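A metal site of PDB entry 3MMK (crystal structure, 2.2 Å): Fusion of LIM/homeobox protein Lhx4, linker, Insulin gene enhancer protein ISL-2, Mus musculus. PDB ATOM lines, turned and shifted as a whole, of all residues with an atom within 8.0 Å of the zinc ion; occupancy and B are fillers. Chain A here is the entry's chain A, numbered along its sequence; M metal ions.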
ATOM      1  N   LYS A  35     -11.626  32.529 -13.183  1.00  0.00           N
ATOM      2  CA  LYS A  35     -12.362  31.280 -13.228  1.00  0.00           C
ATOM      3  C   LYS A  35     -11.483  30.151 -13.782  1.00  0.00           C
ATOM      4  O   LYS A  35     -10.624  30.390 -14.627  1.00  0.00           O
ATOM      5  CB  LYS A  35     -13.627  31.423 -14.070  1.00  0.00           C
ATOM      6  CG  LYS A  35     -14.588  32.499 -13.576  1.00  0.00           C
ATOM      7  N   CYS A  36     -11.705  28.940 -13.290  1.00  0.00           N
ATOM      8  CA  CYS A  36     -10.949  27.777 -13.728  1.00  0.00           C
ATOM      9  C   CYS A  36     -11.149  27.515 -15.220  1.00  0.00           C
ATOM     10  O   CYS A  36     -12.285  27.511 -15.708  1.00  0.00           O
ATOM     11  CB  CYS A  36     -11.340  26.533 -12.939  1.00  0.00           C
ATOM     12  SG  CYS A  36     -10.536  25.017 -13.504  1.00  0.00           S
ATOM     13  N   ALA A  37     -10.055  27.304 -15.929  1.00  0.00           N
ATOM     14  CA  ALA A  37     -10.111  27.036 -17.372  1.00  0.00           C
ATOM     15  C   ALA A  37     -10.876  25.752 -17.666  1.00  0.00           C
ATOM     16  O   ALA A  37     -11.477  25.620 -18.733  1.00  0.00           O
ATOM     17  CB  ALA A  37      -8.700  26.958 -17.939  1.00  0.00           C
ATOM     18  N   ASP A  38     -10.839  24.811 -16.729  1.00  0.00           N
ATOM     19  CA  ASP A  38     -11.486  23.516 -16.930  1.00  0.00           C
ATOM     20  C   ASP A  38     -12.980  23.541 -16.618  1.00  0.00           C
ATOM     21  O   ASP A  38     -13.805  23.337 -17.500  1.00  0.00           O
ATOM     22  CB  ASP A  38     -10.797  22.434 -16.098  1.00  0.00           C
ATOM     23  CG  ASP A  38      -9.493  21.968 -16.713  1.00  0.00           C
ATOM     24  OD1 ASP A  38      -9.210  22.340 -17.878  1.00  0.00           O
ATOM     25  OD2 ASP A  38      -8.735  21.228 -16.042  1.00  0.00           O
ATOM     26  N   CYS A  39     -13.319  23.796 -15.355  1.00  0.00           N
ATOM     27  CA  CYS A  39     -14.703  23.697 -14.908  1.00  0.00           C
ATOM     28  C   CYS A  39     -15.420  25.042 -14.842  1.00  0.00           C
ATOM     29  O   CYS A  39     -16.522  25.141 -14.287  1.00  0.00           O
ATOM     30  CB  CYS A  39     -14.770  23.020 -13.535  1.00  0.00           C
ATOM     31  SG  CYS A  39     -14.265  24.087 -12.173  1.00  0.00           S
ATOM     32  N   GLN A  40     -14.801  26.072 -15.398  1.00  0.00           N
ATOM     33  CA  GLN A  40     -15.386  27.409 -15.415  1.00  0.00           C
ATOM     34  C   GLN A  40     -15.999  27.783 -14.068  1.00  0.00           C
ATOM     35  O   GLN A  40     -17.145  28.219 -14.007  1.00  0.00           O
ATOM     36  CB  GLN A  40     -16.436  27.527 -16.531  1.00  0.00           C
ATOM     37  N   MET A  41     -15.233  27.605 -13.002  1.00  0.00           N
ATOM     38  CA  MET A  41     -15.702  27.956 -11.661  1.00  0.00           C
ATOM     39  C   MET A  41     -14.932  29.140 -11.109  1.00  0.00           C
ATOM     40  O   MET A  41     -13.709  29.223 -11.256  1.00  0.00           O
ATOM     41  CB  MET A  41     -15.566  26.755 -10.717  1.00  0.00           C
ATOM     42  N   GLN A  42     -15.648  30.058 -10.465  1.00  0.00           N
ATOM     43  CA  GLN A  42     -15.030  31.231  -9.872  1.00  0.00           C
ATOM     44  C   GLN A  42     -13.984  30.824  -8.841  1.00  0.00           C
ATOM     45  O   GLN A  42     -14.205  29.889  -8.060  1.00  0.00           O
ATOM     46  N   LEU A  43     -12.849  31.510  -8.840  1.00  0.00           N
ATOM     47  CA  LEU A  43     -11.771  31.222  -7.905  1.00  0.00           C
ATOM     48  C   LEU A  43     -11.741  32.253  -6.777  1.00  0.00           C
ATOM     49  O   LEU A  43     -11.174  33.326  -6.925  1.00  0.00           O
ATOM     50  CB  LEU A  43     -10.421  31.192  -8.629  1.00  0.00           C
ATOM     51  CG  LEU A  43     -10.280  30.183  -9.779  1.00  0.00           C
ATOM     52  CD1 LEU A  43      -8.910  30.300 -10.416  1.00  0.00           C
ATOM     53  CD2 LEU A  43     -10.529  28.762  -9.292  1.00  0.00           C
ATOM     54  N   VAL A  54      -5.489  29.674 -15.671  1.00  0.00           N
ATOM     55  CA  VAL A  54      -5.712  29.498 -14.241  1.00  0.00           C
ATOM     56  C   VAL A  54      -6.646  28.324 -13.943  1.00  0.00           C
ATOM     57  O   VAL A  54      -7.591  28.060 -14.695  1.00  0.00           O
ATOM     58  CB  VAL A  54      -6.263  30.783 -13.594  1.00  0.00           C
ATOM     59  CG1 VAL A  54      -5.204  31.878 -13.637  1.00  0.00           C
ATOM     60  CG2 VAL A  54      -7.524  31.241 -14.294  1.00  0.00           C
ATOM     61  N   TYR A  55      -6.382  27.613 -12.853  1.00  0.00           N
ATOM     62  CA  TYR A  55      -7.151  26.433 -12.509  1.00  0.00           C
ATOM     63  C   TYR A  55      -7.484  26.380 -11.018  1.00  0.00           C
ATOM     64  O   TYR A  55      -6.774  26.958 -10.192  1.00  0.00           O
ATOM     65  CB  TYR A  55      -6.368  25.173 -12.888  1.00  0.00           C
ATOM     66  CG  TYR A  55      -5.918  25.109 -14.326  1.00  0.00           C
ATOM     67  CD1 TYR A  55      -6.643  24.385 -15.271  1.00  0.00           C
ATOM     68  CD2 TYR A  55      -4.765  25.759 -14.747  1.00  0.00           C
ATOM     69  CE1 TYR A  55      -6.234  24.316 -16.591  1.00  0.00           C
ATOM     70  CE2 TYR A  55      -4.352  25.699 -16.066  1.00  0.00           C
ATOM     71  CZ  TYR A  55      -5.090  24.978 -16.977  1.00  0.00           C
ATOM     72  OH  TYR A  55      -4.686  24.899 -18.298  1.00  0.00           O
ATOM     73  N   CYS A  56      -8.561  25.692 -10.678  1.00  0.00           N
ATOM     74  CA  CYS A  56      -8.861  25.411  -9.277  1.00  0.00           C
ATOM     75  C   CYS A  56      -7.947  24.285  -8.785  1.00  0.00           C
ATOM     76  O   CYS A  56      -7.293  23.615  -9.588  1.00  0.00           O
ATOM     77  CB  CYS A  56     -10.329  25.018  -9.110  1.00  0.00           C
ATOM     78  SG  CYS A  56     -10.700  23.331  -9.633  1.00  0.00           S
ATOM     79  N   LYS A  57      -7.910  24.077  -7.472  1.00  0.00           N
ATOM     80  CA  LYS A  57      -6.998  23.096  -6.881  1.00  0.00           C
ATOM     81  C   LYS A  57      -7.207  21.679  -7.418  1.00  0.00           C
ATOM     82  O   LYS A  57      -6.246  20.953  -7.670  1.00  0.00           O
ATOM     83  CB  LYS A  57      -7.117  23.104  -5.359  1.00  0.00           C
ATOM     84  N   GLU A  58      -8.464  21.281  -7.582  1.00  0.00           N
ATOM     85  CA  GLU A  58      -8.799  19.935  -8.025  1.00  0.00           C
ATOM     86  C   GLU A  58      -8.393  19.704  -9.478  1.00  0.00           C
ATOM     87  O   GLU A  58      -7.683  18.748  -9.788  1.00  0.00           O
ATOM     88  CB  GLU A  58     -10.289  19.661  -7.843  1.00  0.00           C
ATOM     89  N   ASP A  59      -8.836  20.587 -10.365  1.00  0.00           N
ATOM     90  CA  ASP A  59      -8.559  20.460 -11.800  1.00  0.00           C
ATOM     91  C   ASP A  59      -7.082  20.657 -12.129  1.00  0.00           C
ATOM     92  O   ASP A  59      -6.618  20.217 -13.178  1.00  0.00           O
ATOM     93  CB  ASP A  59      -9.406  21.448 -12.606  1.00  0.00           C
ATOM     94  CG  ASP A  59     -10.754  20.885 -12.983  1.00  0.00           C
ATOM     95  OD1 ASP A  59     -10.899  19.644 -13.013  1.00  0.00           O
ATOM     96  OD2 ASP A  59     -11.684  21.681 -13.257  1.00  0.00           O
ATOM     97  N   PHE A  60      -6.347  21.304 -11.231  1.00  0.00           N
ATOM     98  CA  PHE A  60      -4.917  21.530 -11.435  1.00  0.00           C
ATOM     99  C   PHE A  60      -4.119  20.271 -11.136  1.00  0.00           C
ATOM    100  O   PHE A  60      -3.253  19.865 -11.920  1.00  0.00           O
ATOM    101  CB  PHE A  60      -4.421  22.682 -10.559  1.00  0.00           C
ATOM    102  CG  PHE A  60      -2.940  22.937 -10.651  1.00  0.00           C
ATOM    103  CD1 PHE A  60      -2.421  23.694 -11.686  1.00  0.00           C
ATOM    104  CD2 PHE A  60      -2.068  22.412  -9.709  1.00  0.00           C
ATOM    105  CE1 PHE A  60      -1.061  23.929 -11.774  1.00  0.00           C
ATOM    106  CE2 PHE A  60      -0.712  22.637  -9.799  1.00  0.00           C
ATOM    107  CZ  PHE A  60      -0.202  23.398 -10.832  1.00  0.00           C
HETATM  108 ZN    ZN M   1     -11.783  23.658 -11.805  1.00  0.00          ZN
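Within 4 Å of the zinc ion: Cys 36, Cys 39, Cys 56 and Asp 59.
N of Glu 58 sits close to SG of Cys 56 (3.7 Å). SG of Cys 36 sits close to N of Asp 38. The backbone NH (N) of Cys 36 lies within hydrogen-bond range of the backbone carbonyl oxygen (O) of Met 41 (2.9 Å). SG of Cys 39 lies close to N of Met 41 (3.7 Å).
The side-chain sulfur (SG) of Cys 56 is bound to the zinc ion (2.4 Å). The side-chain carboxylate (OD2) of Asp 59 binds the zinc ion (2.5 Å). The zinc ion is bound by the side-chain sulfur (SG) of Cys 36, at 2.5 Å. The zinc ion is bound by the side-chain sulfur (SG) of Cys 39 (2.5 Å). The zinc ion has four donor atoms within binding distance.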
